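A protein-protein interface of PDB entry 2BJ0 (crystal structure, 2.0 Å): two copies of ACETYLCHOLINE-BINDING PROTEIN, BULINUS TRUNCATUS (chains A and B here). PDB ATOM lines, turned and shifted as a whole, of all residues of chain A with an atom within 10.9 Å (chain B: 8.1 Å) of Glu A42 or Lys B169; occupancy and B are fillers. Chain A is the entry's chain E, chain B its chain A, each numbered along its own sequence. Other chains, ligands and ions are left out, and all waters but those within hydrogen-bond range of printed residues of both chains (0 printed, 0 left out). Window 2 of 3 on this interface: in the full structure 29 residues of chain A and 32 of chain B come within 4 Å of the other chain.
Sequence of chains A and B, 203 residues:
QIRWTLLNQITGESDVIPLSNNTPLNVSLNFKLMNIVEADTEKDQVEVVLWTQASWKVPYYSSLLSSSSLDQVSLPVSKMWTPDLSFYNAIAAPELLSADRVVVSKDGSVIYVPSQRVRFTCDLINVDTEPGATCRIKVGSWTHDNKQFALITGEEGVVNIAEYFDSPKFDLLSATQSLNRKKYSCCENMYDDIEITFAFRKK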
ATOM      1  N   GLU A  38      13.154  32.196 -12.822  1.00  0.00           N
ATOM      2  CA  GLU A  38      14.498  32.330 -13.415  1.00  0.00           C
ATOM      3  C   GLU A  38      15.077  30.936 -13.491  1.00  0.00           C
ATOM      4  O   GLU A  38      14.927  30.155 -12.560  1.00  0.00           O
ATOM      5  CB  GLU A  38      15.482  33.175 -12.573  1.00  0.00           C
ATOM      6  CG  GLU A  38      15.083  34.601 -12.188  1.00  0.00           C
ATOM      7  CD  GLU A  38      15.173  35.652 -13.315  1.00  0.00           C
ATOM      8  OE1 GLU A  38      15.851  35.412 -14.364  1.00  0.00           O
ATOM      9  OE2 GLU A  38      14.559  36.744 -13.141  1.00  0.00           O
ATOM     10  N   ALA A  39      15.702  30.622 -14.617  1.00  0.00           N
ATOM     11  CA  ALA A  39      16.518  29.417 -14.726  1.00  0.00           C
ATOM     12  C   ALA A  39      17.732  29.812 -15.535  1.00  0.00           C
ATOM     13  O   ALA A  39      17.683  29.817 -16.762  1.00  0.00           O
ATOM     14  CB  ALA A  39      15.749  28.273 -15.377  1.00  0.00           C
ATOM     15  N   ASP A  40      18.800  30.169 -14.825  1.00  0.00           N
ATOM     16  CA  ASP A  40      20.050  30.662 -15.398  1.00  0.00           C
ATOM     17  C   ASP A  40      21.080  29.540 -15.577  1.00  0.00           C
ATOM     18  O   ASP A  40      21.710  29.086 -14.608  1.00  0.00           O
ATOM     19  CB  ASP A  40      20.619  31.754 -14.495  1.00  0.00           C
ATOM     20  CG  ASP A  40      21.715  32.562 -15.166  1.00  0.00           C
ATOM     21  OD1 ASP A  40      22.427  32.035 -16.035  1.00  0.00           O
ATOM     22  OD2 ASP A  40      21.947  33.751 -14.874  1.00  0.00           O
ATOM     23  N   THR A  41      21.267  29.142 -16.834  1.00  0.00           N
ATOM     24  CA  THR A  41      22.069  27.989 -17.174  1.00  0.00           C
ATOM     25  C   THR A  41      23.546  28.336 -17.168  1.00  0.00           C
ATOM     26  O   THR A  41      24.366  27.450 -17.054  1.00  0.00           O
ATOM     27  CB  THR A  41      21.668  27.429 -18.535  1.00  0.00           C
ATOM     28  OG1 THR A  41      21.773  28.467 -19.509  1.00  0.00           O
ATOM     29  CG2 THR A  41      20.166  27.073 -18.566  1.00  0.00           C
ATOM     30  N   GLU A  42      23.879  29.623 -17.280  1.00  0.00           N
ATOM     31  CA  GLU A  42      25.264  30.063 -17.146  1.00  0.00           C
ATOM     32  C   GLU A  42      25.720  30.055 -15.694  1.00  0.00           C
ATOM     33  O   GLU A  42      26.828  29.601 -15.395  1.00  0.00           O
ATOM     34  CB  GLU A  42      25.468  31.452 -17.757  1.00  0.00           C
ATOM     35  CG  GLU A  42      25.785  31.454 -19.249  1.00  0.00           C
ATOM     36  CD  GLU A  42      25.476  32.793 -19.938  1.00  0.00           C
ATOM     37  OE1 GLU A  42      24.801  33.675 -19.334  1.00  0.00           O
ATOM     38  OE2 GLU A  42      25.902  32.977 -21.108  1.00  0.00           O
ATOM     39  N   LYS A  43      24.865  30.549 -14.799  1.00  0.00           N
ATOM     40  CA  LYS A  43      25.122  30.558 -13.351  1.00  0.00           C
ATOM     41  C   LYS A  43      24.708  29.299 -12.591  1.00  0.00           C
ATOM     42  O   LYS A  43      25.184  29.079 -11.463  1.00  0.00           O
ATOM     43  CB  LYS A  43      24.411  31.744 -12.698  1.00  0.00           C
ATOM     44  CG  LYS A  43      24.971  33.069 -13.092  1.00  0.00           C
ATOM     45  CD  LYS A  43      24.227  34.226 -12.430  1.00  0.00           C
ATOM     46  CE  LYS A  43      24.786  35.555 -12.914  1.00  0.00           C
ATOM     47  NZ  LYS A  43      26.273  35.663 -12.666  1.00  0.00           N
ATOM     48  N   ASP A  44      23.827  28.490 -13.177  1.00  0.00           N
ATOM     49  CA  ASP A  44      23.220  27.331 -12.510  1.00  0.00           C
ATOM     50  C   ASP A  44      22.457  27.742 -11.261  1.00  0.00           C
ATOM     51  O   ASP A  44      22.820  27.323 -10.147  1.00  0.00           O
ATOM     52  CB  ASP A  44      24.280  26.263 -12.148  1.00  0.00           C
ATOM     53  CG  ASP A  44      24.552  25.289 -13.306  1.00  0.00           C
ATOM     54  OD1 ASP A  44      23.692  25.195 -14.216  1.00  0.00           O
ATOM     55  OD2 ASP A  44      25.598  24.562 -13.372  1.00  0.00           O
ATOM     56  N   GLN A  45      21.407  28.561 -11.449  1.00  0.00           N
ATOM     57  CA  GLN A  45      20.647  29.151 -10.360  1.00  0.00           C
ATOM     58  C   GLN A  45      19.215  29.290 -10.836  1.00  0.00           C
ATOM     59  O   GLN A  45      18.974  29.664 -11.973  1.00  0.00           O
ATOM     60  CB  GLN A  45      21.168  30.540 -10.012  1.00  0.00           C
ATOM     61  CG  GLN A  45      22.568  30.508  -9.418  1.00  0.00           C
ATOM     62  CD  GLN A  45      23.134  31.857  -9.135  1.00  0.00           C
ATOM     63  OE1 GLN A  45      22.450  32.901  -9.288  1.00  0.00           O
ATOM     64  NE2 GLN A  45      24.399  31.868  -8.712  1.00  0.00           N
ATOM     65  N   VAL A  46      18.295  28.944  -9.955  1.00  0.00           N
ATOM     66  CA  VAL A  46      16.852  28.931 -10.259  1.00  0.00           C
ATOM     67  C   VAL A  46      16.177  29.842  -9.239  1.00  0.00           C
ATOM     68  O   VAL A  46      16.631  29.914  -8.100  1.00  0.00           O
ATOM     69  CB  VAL A  46      16.273  27.493 -10.102  1.00  0.00           C
ATOM     70  CG1 VAL A  46      14.752  27.460 -10.397  1.00  0.00           C
ATOM     71  CG2 VAL A  46      16.965  26.579 -11.074  1.00  0.00           C
ATOM     72  N   ILE A  91      20.442  30.964  -1.664  1.00  0.00           N
ATOM     73  CA  ILE A  91      21.599  31.770  -2.020  1.00  0.00           C
ATOM     74  C   ILE A  91      21.279  33.279  -2.098  1.00  0.00           C
ATOM     75  O   ILE A  91      22.135  34.092  -2.400  1.00  0.00           O
ATOM     76  CB  ILE A  91      22.246  31.228  -3.354  1.00  0.00           C
ATOM     77  CG1 ILE A  91      21.309  31.363  -4.545  1.00  0.00           C
ATOM     78  CG2 ILE A  91      22.668  29.760  -3.183  1.00  0.00           C
ATOM     79  CD1 ILE A  91      21.995  31.102  -5.882  1.00  0.00           C
ATOM     80  N   PHE A 120      18.087  29.576  -5.510  1.00  0.00           N
ATOM     81  CA  PHE A 120      19.001  28.529  -5.103  1.00  0.00           C
ATOM     82  C   PHE A 120      19.776  28.048  -6.323  1.00  0.00           C
ATOM     83  O   PHE A 120      19.414  28.332  -7.454  1.00  0.00           O
ATOM     84  CB  PHE A 120      18.273  27.374  -4.393  1.00  0.00           C
ATOM     85  CG  PHE A 120      17.078  26.891  -5.118  1.00  0.00           C
ATOM     86  CD1 PHE A 120      15.867  27.574  -5.012  1.00  0.00           C
ATOM     87  CD2 PHE A 120      17.156  25.780  -5.955  1.00  0.00           C
ATOM     88  CE1 PHE A 120      14.769  27.149  -5.722  1.00  0.00           C
ATOM     89  CE2 PHE A 120      16.042  25.333  -6.673  1.00  0.00           C
ATOM     90  CZ  PHE A 120      14.852  26.017  -6.554  1.00  0.00           C
ATOM     91  N   THR A 121      20.874  27.359  -6.039  1.00  0.00           N
ATOM     92  CA  THR A 121      21.730  26.715  -7.022  1.00  0.00           C
ATOM     93  C   THR A 121      21.094  25.417  -7.492  1.00  0.00           C
ATOM     94  O   THR A 121      20.643  24.630  -6.680  1.00  0.00           O
ATOM     95  CB  THR A 121      23.085  26.432  -6.337  1.00  0.00           C
ATOM     96  OG1 THR A 121      23.849  27.640  -6.359  1.00  0.00           O
ATOM     97  CG2 THR A 121      23.911  25.500  -7.147  1.00  0.00           C
ATOM     98  N   CYS A 122      21.070  25.204  -8.809  1.00  0.00           N
ATOM     99  CA  CYS A 122      20.624  23.952  -9.391  1.00  0.00           C
ATOM    100  C   CYS A 122      21.427  23.675 -10.653  1.00  0.00           C
ATOM    101  O   CYS A 122      21.584  24.576 -11.467  1.00  0.00           O
ATOM    102  CB  CYS A 122      19.152  24.063  -9.775  1.00  0.00           C
ATOM    103  SG  CYS A 122      18.433  22.493 -10.305  1.00  0.00           S
ATOM    104  N   ASP A 123      21.898  22.440 -10.842  1.00  0.00           N
ATOM    105  CA  ASP A 123      22.569  22.065 -12.103  1.00  0.00           C
ATOM    106  C   ASP A 123      21.554  21.975 -13.215  1.00  0.00           C
ATOM    107  O   ASP A 123      20.727  21.069 -13.244  1.00  0.00           O
ATOM    108  CB  ASP A 123      23.313  20.727 -11.990  1.00  0.00           C
ATOM    109  CG  ASP A 123      24.192  20.442 -13.204  1.00  0.00           C
ATOM    110  OD1 ASP A 123      24.086  21.160 -14.243  1.00  0.00           O
ATOM    111  OD2 ASP A 123      25.056  19.522 -13.198  1.00  0.00           O
ATOM    112  N   LEU A 124      21.633  22.908 -14.141  1.00  0.00           N
ATOM    113  CA  LEU A 124      20.614  23.034 -15.172  1.00  0.00           C
ATOM    114  C   LEU A 124      21.110  22.535 -16.514  1.00  0.00           C
ATOM    115  O   LEU A 124      20.513  22.841 -17.549  1.00  0.00           O
ATOM    116  CB  LEU A 124      20.227  24.508 -15.329  1.00  0.00           C
ATOM    117  CG  LEU A 124      19.451  25.158 -14.190  1.00  0.00           C
ATOM    118  CD1 LEU A 124      19.252  26.603 -14.569  1.00  0.00           C
ATOM    119  CD2 LEU A 124      18.128  24.432 -13.945  1.00  0.00           C
ATOM    120  N   ILE A 125      22.211  21.781 -16.508  1.00  0.00           N
ATOM    121  CA  ILE A 125      22.720  21.215 -17.755  1.00  0.00           C
ATOM    122  C   ILE A 125      21.647  20.506 -18.592  1.00  0.00           C
ATOM    123  O   ILE A 125      21.716  20.534 -19.823  1.00  0.00           O
ATOM    124  CB  ILE A 125      23.936  20.284 -17.495  1.00  0.00           C
ATOM    125  CG1 ILE A 125      24.619  19.961 -18.820  1.00  0.00           C
ATOM    126  CG2 ILE A 125      23.492  19.004 -16.773  1.00  0.00           C
ATOM    127  CD1 ILE A 125      26.047  19.525 -18.657  1.00  0.00           C
ATOM    128  N   ASN A 126      20.664  19.869 -17.943  1.00  0.00           N
ATOM    129  CA  ASN A 126      19.614  19.123 -18.664  1.00  0.00           C
ATOM    130  C   ASN A 126      18.252  19.829 -18.767  1.00  0.00           C
ATOM    131  O   ASN A 126      17.251  19.196 -19.077  1.00  0.00           O
ATOM    132  CB  ASN A 126      19.405  17.735 -18.050  1.00  0.00           C
ATOM    133  CG  ASN A 126      20.531  16.752 -18.404  1.00  0.00           C
ATOM    134  OD1 ASN A 126      21.183  16.869 -19.424  1.00  0.00           O
ATOM    135  ND2 ASN A 126      20.735  15.782 -17.558  1.00  0.00           N
ATOM    136  N   VAL A 127      18.220  21.135 -18.533  1.00  0.00           N
ATOM    137  CA  VAL A 127      16.939  21.862 -18.477  1.00  0.00           C
ATOM    138  C   VAL A 127      16.215  21.890 -19.804  1.00  0.00           C
ATOM    139  O   VAL A 127      15.006  22.070 -19.840  1.00  0.00           O
ATOM    140  CB  VAL A 127      17.101  23.303 -17.930  1.00  0.00           C
ATOM    141  CG1 VAL A 127      17.562  24.236 -19.006  1.00  0.00           C
ATOM    142  CG2 VAL A 127      15.797  23.782 -17.319  1.00  0.00           C
ATOM    143  N   LYS A 202      12.466  23.383 -20.212  1.00  0.00           N
ATOM    144  CA  LYS A 202      11.967  24.476 -21.056  1.00  0.00           C
ATOM    145  C   LYS A 202      10.790  24.016 -21.911  1.00  0.00           C
ATOM    146  O   LYS A 202      10.772  22.878 -22.371  1.00  0.00           O
ATOM    147  CB  LYS A 202      13.054  24.996 -21.977  1.00  0.00           C
ATOM    148  CG  LYS A 202      14.102  25.845 -21.301  1.00  0.00           C
ATOM    149  CD  LYS A 202      14.922  26.550 -22.363  1.00  0.00           C
ATOM    150  CE  LYS A 202      16.193  27.155 -21.815  1.00  0.00           C
ATOM    151  NZ  LYS A 202      16.725  28.078 -22.876  1.00  0.00           N
ATOM    152  N   ASN B  35      28.839  27.536  -0.683  1.00  0.00           N
ATOM    153  CA  ASN B  35      28.729  27.656  -2.099  1.00  0.00           C
ATOM    154  C   ASN B  35      29.536  28.897  -2.567  1.00  0.00           C
ATOM    155  O   ASN B  35      29.723  29.832  -1.805  1.00  0.00           O
ATOM    156  CB  ASN B  35      27.269  27.821  -2.484  1.00  0.00           C
ATOM    157  CG  ASN B  35      26.946  27.468  -3.910  1.00  0.00           C
ATOM    158  OD1 ASN B  35      27.839  27.209  -4.714  1.00  0.00           O
ATOM    159  ND2 ASN B  35      25.657  27.436  -4.239  1.00  0.00           N
ATOM    160  N   ILE B  36      29.984  28.876  -3.780  1.00  0.00           N
ATOM    161  CA  ILE B  36      30.608  30.030  -4.431  1.00  0.00           C
ATOM    162  C   ILE B  36      29.586  30.337  -5.483  1.00  0.00           C
ATOM    163  O   ILE B  36      29.442  29.569  -6.427  1.00  0.00           O
ATOM    164  CB  ILE B  36      31.962  29.733  -5.034  1.00  0.00           C
ATOM    165  CG1 ILE B  36      33.023  29.522  -3.940  1.00  0.00           C
ATOM    166  CG2 ILE B  36      32.376  30.859  -5.964  1.00  0.00           C
ATOM    167  CD1 ILE B  36      34.389  29.179  -4.492  1.00  0.00           C
ATOM    168  N   VAL B  37      28.841  31.444  -5.339  1.00  0.00           N
ATOM    169  CA  VAL B  37      27.704  31.734  -6.268  1.00  0.00           C
ATOM    170  C   VAL B  37      27.994  32.678  -7.442  1.00  0.00           C
ATOM    171  O   VAL B  37      27.215  32.720  -8.402  1.00  0.00           O
ATOM    172  CB  VAL B  37      26.463  32.165  -5.465  1.00  0.00           C
ATOM    173  CG1 VAL B  37      25.944  31.000  -4.645  1.00  0.00           C
ATOM    174  CG2 VAL B  37      26.780  33.344  -4.568  1.00  0.00           C
ATOM    175  N   GLU B  38      29.085  33.434  -7.373  1.00  0.00           N
ATOM    176  CA  GLU B  38      29.595  34.173  -8.510  1.00  0.00           C
ATOM    177  C   GLU B  38      31.128  34.154  -8.462  1.00  0.00           C
ATOM    178  O   GLU B  38      31.709  34.249  -7.394  1.00  0.00           O
ATOM    179  CB  GLU B  38      29.126  35.618  -8.447  1.00  0.00           C
ATOM    180  CG  GLU B  38      29.415  36.381  -9.722  1.00  0.00           C
ATOM    181  CD  GLU B  38      28.547  37.624  -9.856  1.00  0.00           C
ATOM    182  OE1 GLU B  38      28.553  38.459  -8.914  1.00  0.00           O
ATOM    183  OE2 GLU B  38      27.852  37.773 -10.901  1.00  0.00           O
ATOM    184  N   ALA B  39      31.775  34.016  -9.614  1.00  0.00           N
ATOM    185  CA  ALA B  39      33.187  34.379  -9.721  1.00  0.00           C
ATOM    186  C   ALA B  39      33.376  35.094 -11.040  1.00  0.00           C
ATOM    187  O   ALA B  39      33.481  34.468 -12.098  1.00  0.00           O
ATOM    188  CB  ALA B  39      34.097  33.163  -9.597  1.00  0.00           C
ATOM    189  N   VAL B 127      41.685  31.174 -12.170  1.00  0.00           N
ATOM    190  CA  VAL B 127      40.517  30.426 -11.692  1.00  0.00           C
ATOM    191  C   VAL B 127      40.247  29.216 -12.556  1.00  0.00           C
ATOM    192  O   VAL B 127      39.516  28.294 -12.172  1.00  0.00           O
ATOM    193  CB  VAL B 127      39.229  31.333 -11.569  1.00  0.00           C
ATOM    194  CG1 VAL B 127      38.624  31.632 -12.920  1.00  0.00           C
ATOM    195  CG2 VAL B 127      38.201  30.703 -10.641  1.00  0.00           C
ATOM    196  N   PHE B 165      30.235  22.073   1.406  1.00  0.00           N
ATOM    197  CA  PHE B 165      30.356  22.774   0.140  1.00  0.00           C
ATOM    198  C   PHE B 165      29.702  21.984  -1.010  1.00  0.00           C
ATOM    199  O   PHE B 165      29.886  20.769  -1.112  1.00  0.00           O
ATOM    200  CB  PHE B 165      31.827  23.085  -0.163  1.00  0.00           C
ATOM    201  CG  PHE B 165      32.017  23.905  -1.396  1.00  0.00           C
ATOM    202  CD1 PHE B 165      32.113  23.296  -2.650  1.00  0.00           C
ATOM    203  CD2 PHE B 165      32.046  25.292  -1.320  1.00  0.00           C
ATOM    204  CE1 PHE B 165      32.249  24.061  -3.811  1.00  0.00           C
ATOM    205  CE2 PHE B 165      32.192  26.071  -2.479  1.00  0.00           C
ATOM    206  CZ  PHE B 165      32.310  25.456  -3.721  1.00  0.00           C
ATOM    207  N   ASP B 166      28.958  22.671  -1.883  1.00  0.00           N
ATOM    208  CA  ASP B 166      28.280  22.016  -3.001  1.00  0.00           C
ATOM    209  C   ASP B 166      28.099  23.058  -4.089  1.00  0.00           C
ATOM    210  O   ASP B 166      27.427  24.064  -3.862  1.00  0.00           O
ATOM    211  CB  ASP B 166      26.909  21.497  -2.515  1.00  0.00           C
ATOM    212  CG  ASP B 166      26.255  20.466  -3.459  1.00  0.00           C
ATOM    213  OD1 ASP B 166      26.783  20.149  -4.563  1.00  0.00           O
ATOM    214  OD2 ASP B 166      25.170  19.901  -3.138  1.00  0.00           O
ATOM    215  N   SER B 167      28.692  22.836  -5.263  1.00  0.00           N
ATOM    216  CA  SER B 167      28.439  23.682  -6.424  1.00  0.00           C
ATOM    217  C   SER B 167      28.504  22.862  -7.712  1.00  0.00           C
ATOM    218  O   SER B 167      29.392  22.033  -7.828  1.00  0.00           O
ATOM    219  CB  SER B 167      29.476  24.809  -6.481  1.00  0.00           C
ATOM    220  OG  SER B 167      29.483  25.452  -7.749  1.00  0.00           O
ATOM    221  N   PRO B 168      27.584  23.063  -8.661  1.00  0.00           N
ATOM    222  CA  PRO B 168      27.736  22.483  -9.992  1.00  0.00           C
ATOM    223  C   PRO B 168      28.756  23.223 -10.845  1.00  0.00           C
ATOM    224  O   PRO B 168      29.201  22.686 -11.851  1.00  0.00           O
ATOM    225  CB  PRO B 168      26.335  22.602 -10.600  1.00  0.00           C
ATOM    226  CG  PRO B 168      25.727  23.782  -9.933  1.00  0.00           C
ATOM    227  CD  PRO B 168      26.309  23.796  -8.540  1.00  0.00           C
ATOM    228  N   LYS B 169      29.171  24.415 -10.409  1.00  0.00           N
ATOM    229  CA  LYS B 169      30.042  25.286 -11.184  1.00  0.00           C
ATOM    230  C   LYS B 169      31.521  25.318 -10.742  1.00  0.00           C
ATOM    231  O   LYS B 169      32.409  25.585 -11.565  1.00  0.00           O
ATOM    232  CB  LYS B 169      29.489  26.694 -11.114  1.00  0.00           C
ATOM    233  CG  LYS B 169      28.268  26.910 -11.997  1.00  0.00           C
ATOM    234  CD  LYS B 169      28.766  27.500 -13.296  1.00  0.00           C
ATOM    235  CE  LYS B 169      28.285  26.720 -14.469  1.00  0.00           C
ATOM    236  NZ  LYS B 169      28.701  27.452 -15.702  1.00  0.00           N
ATOM    237  N   PHE B 170      31.787  25.111  -9.452  1.00  0.00           N
ATOM    238  CA  PHE B 170      33.168  25.240  -8.947  1.00  0.00           C
ATOM    239  C   PHE B 170      33.614  24.075  -8.096  1.00  0.00           C
ATOM    240  O   PHE B 170      32.797  23.481  -7.415  1.00  0.00           O
ATOM    241  CB  PHE B 170      33.316  26.539  -8.133  1.00  0.00           C
ATOM    242  CG  PHE B 170      32.860  27.770  -8.872  1.00  0.00           C
ATOM    243  CD1 PHE B 170      33.673  28.360  -9.841  1.00  0.00           C
ATOM    244  CD2 PHE B 170      31.605  28.319  -8.624  1.00  0.00           C
ATOM    245  CE1 PHE B 170      33.235  29.493 -10.555  1.00  0.00           C
ATOM    246  CE2 PHE B 170      31.164  29.460  -9.320  1.00  0.00           C
ATOM    247  CZ  PHE B 170      31.964  30.031 -10.288  1.00  0.00           C
ATOM    248  N   ASP B 171      34.920  23.764  -8.128  1.00  0.00           N
ATOM    249  CA  ASP B 171      35.551  22.792  -7.227  1.00  0.00           C
ATOM    250  C   ASP B 171      36.219  23.590  -6.121  1.00  0.00           C
ATOM    251  O   ASP B 171      37.045  24.438  -6.414  1.00  0.00           O
ATOM    252  CB  ASP B 171      36.705  22.031  -7.926  1.00  0.00           C
ATOM    253  CG  ASP B 171      36.240  20.957  -8.887  1.00  0.00           C
ATOM    254  OD1 ASP B 171      35.280  20.208  -8.571  1.00  0.00           O
ATOM    255  OD2 ASP B 171      36.798  20.784 -10.005  1.00  0.00           O
ATOM    256  N   LEU B 172      35.899  23.321  -4.863  1.00  0.00           N
ATOM    257  CA  LEU B 172      36.649  23.909  -3.786  1.00  0.00           C
ATOM    258  C   LEU B 172      37.878  23.042  -3.487  1.00  0.00           C
ATOM    259  O   LEU B 172      37.739  21.904  -3.056  1.00  0.00           O
ATOM    260  CB  LEU B 172      35.786  24.004  -2.537  1.00  0.00           C
ATOM    261  CG  LEU B 172      36.377  24.633  -1.285  1.00  0.00           C
ATOM    262  CD1 LEU B 172      36.816  26.078  -1.523  1.00  0.00           C
ATOM    263  CD2 LEU B 172      35.313  24.572  -0.213  1.00  0.00           C
ATOM    264  N   PHE B 200      39.865  27.745  -5.114  1.00  0.00           N
ATOM    265  CA  PHE B 200      38.814  27.132  -5.906  1.00  0.00           C
ATOM    266  C   PHE B 200      39.100  27.265  -7.401  1.00  0.00           C
ATOM    267  O   PHE B 200      39.856  28.132  -7.811  1.00  0.00           O
ATOM    268  CB  PHE B 200      37.445  27.762  -5.550  1.00  0.00           C
ATOM    269  CG  PHE B 200      37.186  29.111  -6.194  1.00  0.00           C
ATOM    270  CD1 PHE B 200      37.819  30.253  -5.730  1.00  0.00           C
ATOM    271  CD2 PHE B 200      36.263  29.231  -7.229  1.00  0.00           C
ATOM    272  CE1 PHE B 200      37.569  31.484  -6.323  1.00  0.00           C
ATOM    273  CE2 PHE B 200      35.999  30.453  -7.815  1.00  0.00           C
ATOM    274  CZ  PHE B 200      36.651  31.578  -7.369  1.00  0.00           C
ATOM    275  N   ARG B 201      38.455  26.449  -8.223  1.00  0.00           N
ATOM    276  CA  ARG B 201      38.639  26.544  -9.661  1.00  0.00           C
ATOM    277  C   ARG B 201      37.310  26.280 -10.379  1.00  0.00           C
ATOM    278  O   ARG B 201      36.389  25.789  -9.763  1.00  0.00           O
ATOM    279  CB  ARG B 201      39.736  25.561 -10.111  1.00  0.00           C
ATOM    280  CG  ARG B 201      39.397  24.099  -9.832  1.00  0.00           C
ATOM    281  CD  ARG B 201      40.260  23.065 -10.569  1.00  0.00           C
ATOM    282  NE  ARG B 201      39.809  21.709 -10.238  1.00  0.00           N
ATOM    283  CZ  ARG B 201      40.624  20.698  -9.947  1.00  0.00           C
ATOM    284  NH1 ARG B 201      41.941  20.880  -9.929  1.00  0.00           N
ATOM    285  NH2 ARG B 201      40.120  19.512  -9.642  1.00  0.00           N
ATOM    286  N   LYS B 202      37.193  26.647 -11.660  1.00  0.00           N
ATOM    287  CA  LYS B 202      36.006  26.301 -12.455  1.00  0.00           C
ATOM    288  C   LYS B 202      35.983  24.781 -12.741  1.00  0.00           C
ATOM    289  O   LYS B 202      37.039  24.173 -12.855  1.00  0.00           O
ATOM    290  CB  LYS B 202      35.965  27.108 -13.759  1.00  0.00           C
ATOM    291  CG  LYS B 202      35.989  28.618 -13.543  1.00  0.00           C
ATOM    292  CD  LYS B 202      36.146  29.410 -14.824  1.00  0.00           C
ATOM    293  CE  LYS B 202      34.844  30.142 -15.175  1.00  0.00           C
ATOM    294  NZ  LYS B 202      35.033  31.385 -16.041  1.00  0.00           N
ATOM    295  N   LYS B 203      34.805  24.168 -12.840  1.00  0.00           N
ATOM    296  CA  LYS B 203      34.719  22.734 -13.182  1.00  0.00           C
ATOM    297  C   LYS B 203      34.990  22.508 -14.666  1.00  0.00           C
ATOM    298  O   LYS B 203      34.776  23.419 -15.479  1.00  0.00           O
ATOM    299  CB  LYS B 203      33.356  22.149 -12.840  1.00  0.00           C
ATOM    300  CG  LYS B 203      33.076  22.095 -11.385  1.00  0.00           C
ATOM    301  CD  LYS B 203      32.049  21.048 -11.069  1.00  0.00           C
ATOM    302  CE  LYS B 203      31.928  20.938  -9.558  1.00  0.00           C
ATOM    303  NZ  LYS B 203      32.129  19.561  -9.077  1.00  0.00           N
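OE2 of Glu B38 is in salt-bridge range of NZ of Lys A43, 3.2 Å away.
O of Glu A42 sits at hydrogen-bond distance from NZ of Lys B169 (2.9 Å).
The backbone carbonyl oxygen (O) of Val B37 is in hydrogen-bond range of the side-chain amide nitrogen (NE2) of Gln A45 (3.0 Å).
The side-chain amide nitrogen (ND2) of Asn B35 lies within hydrogen-bond range of the side-chain hydroxyl (OG1) of Thr A121 (2.8 Å).
Of chain B, only Lys B169 (2.9 Å) comes within 4 Å of Glu A42.
Lys B169 touches just these residues of chain A: Glu A42, Lys A43 and Asp A44.
Ser B167 touches none of the printed residues of chain A.
Pro B168 touches three residues of chain A.
Phe B170 touches none of the printed residues of chain A.
No residue of chain A comes within 4 Å of Lys B203.
Printed residues of chain B within 4 Å of Asp A123: Pro B168 (3.8 Å).
Printed residues of chain A within 4 Å of Asn B35: Ile A91 (3.9 Å) and Thr A121 (2.8 Å).
The nearest residue of chain B that does not touch Glu A42 is Phe B170 (7.3 Å).
The nearest printed residue of chain B that does not touch Lys A43 is Val B37 (5.2 Å).
The backbone carbonyl oxygen (O) of Asp B166 lies close to the side-chain amide oxygen (OD1) of Asn B35 (3.3 Å).
N of Lys A43 lies within hydrogen-bond range of OD1 of Asp A40 (3.1 Å).
The backbone NH of Lys B203 lies within hydrogen-bond range of the backbone carbonyl oxygen of Lys B169.
The backbone NH (N) of Asp A40 is in hydrogen-bond range of the backbone carbonyl oxygen (O) of Gln A45, at 2.9 Å.
The side-chain carboxylate (OD1) of Asp A44 sits at hydrogen-bond distance from the backbone NH (N) of Leu A124 (3.1 Å).
N of Glu A42 is in hydrogen-bond range of OD1 of Asp A40 (3.1 Å).
Printed residues of chain A that touch a printed residue of chain B: Glu A42, Lys A43, Asp A44, Gln A45, Ile A91, Thr A121 and Asp A123.
Of the 18 printed residues of chain B, 5 touch a printed residue of chain A.
Along chain B the printed residues that touch a printed residue of chain A span positions 35 to 169.
Among the printed residues, 11 pairs touch across the chains.
Among the printed residues, Asp or Glu carboxylates within 4 Å of a Lys or Arg side-chain nitrogen of the other chain: Lys A43 with Glu B38 (3.2 Å).
Positions printed for both chains: 38, 39, 127 and 202.
Of the 11 pairs that touch across the chains among the printed residues, none has its exchanged pair printed and touching as well.
Among the printed residues, merely in contact across the chains: Lys A43 with Lys B169 (3.8 Å), Asp A44 with Pro B168 (3.5 Å), Asp A44 with Lys B169 (3.6 Å), Ile A91 with Asn B35 (3.9 Å), Ile A91 with Val B37 (3.8 Å), Thr A121 with Pro B168 (3.3 Å) and Asp A123 with Pro B168 (3.8 Å).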
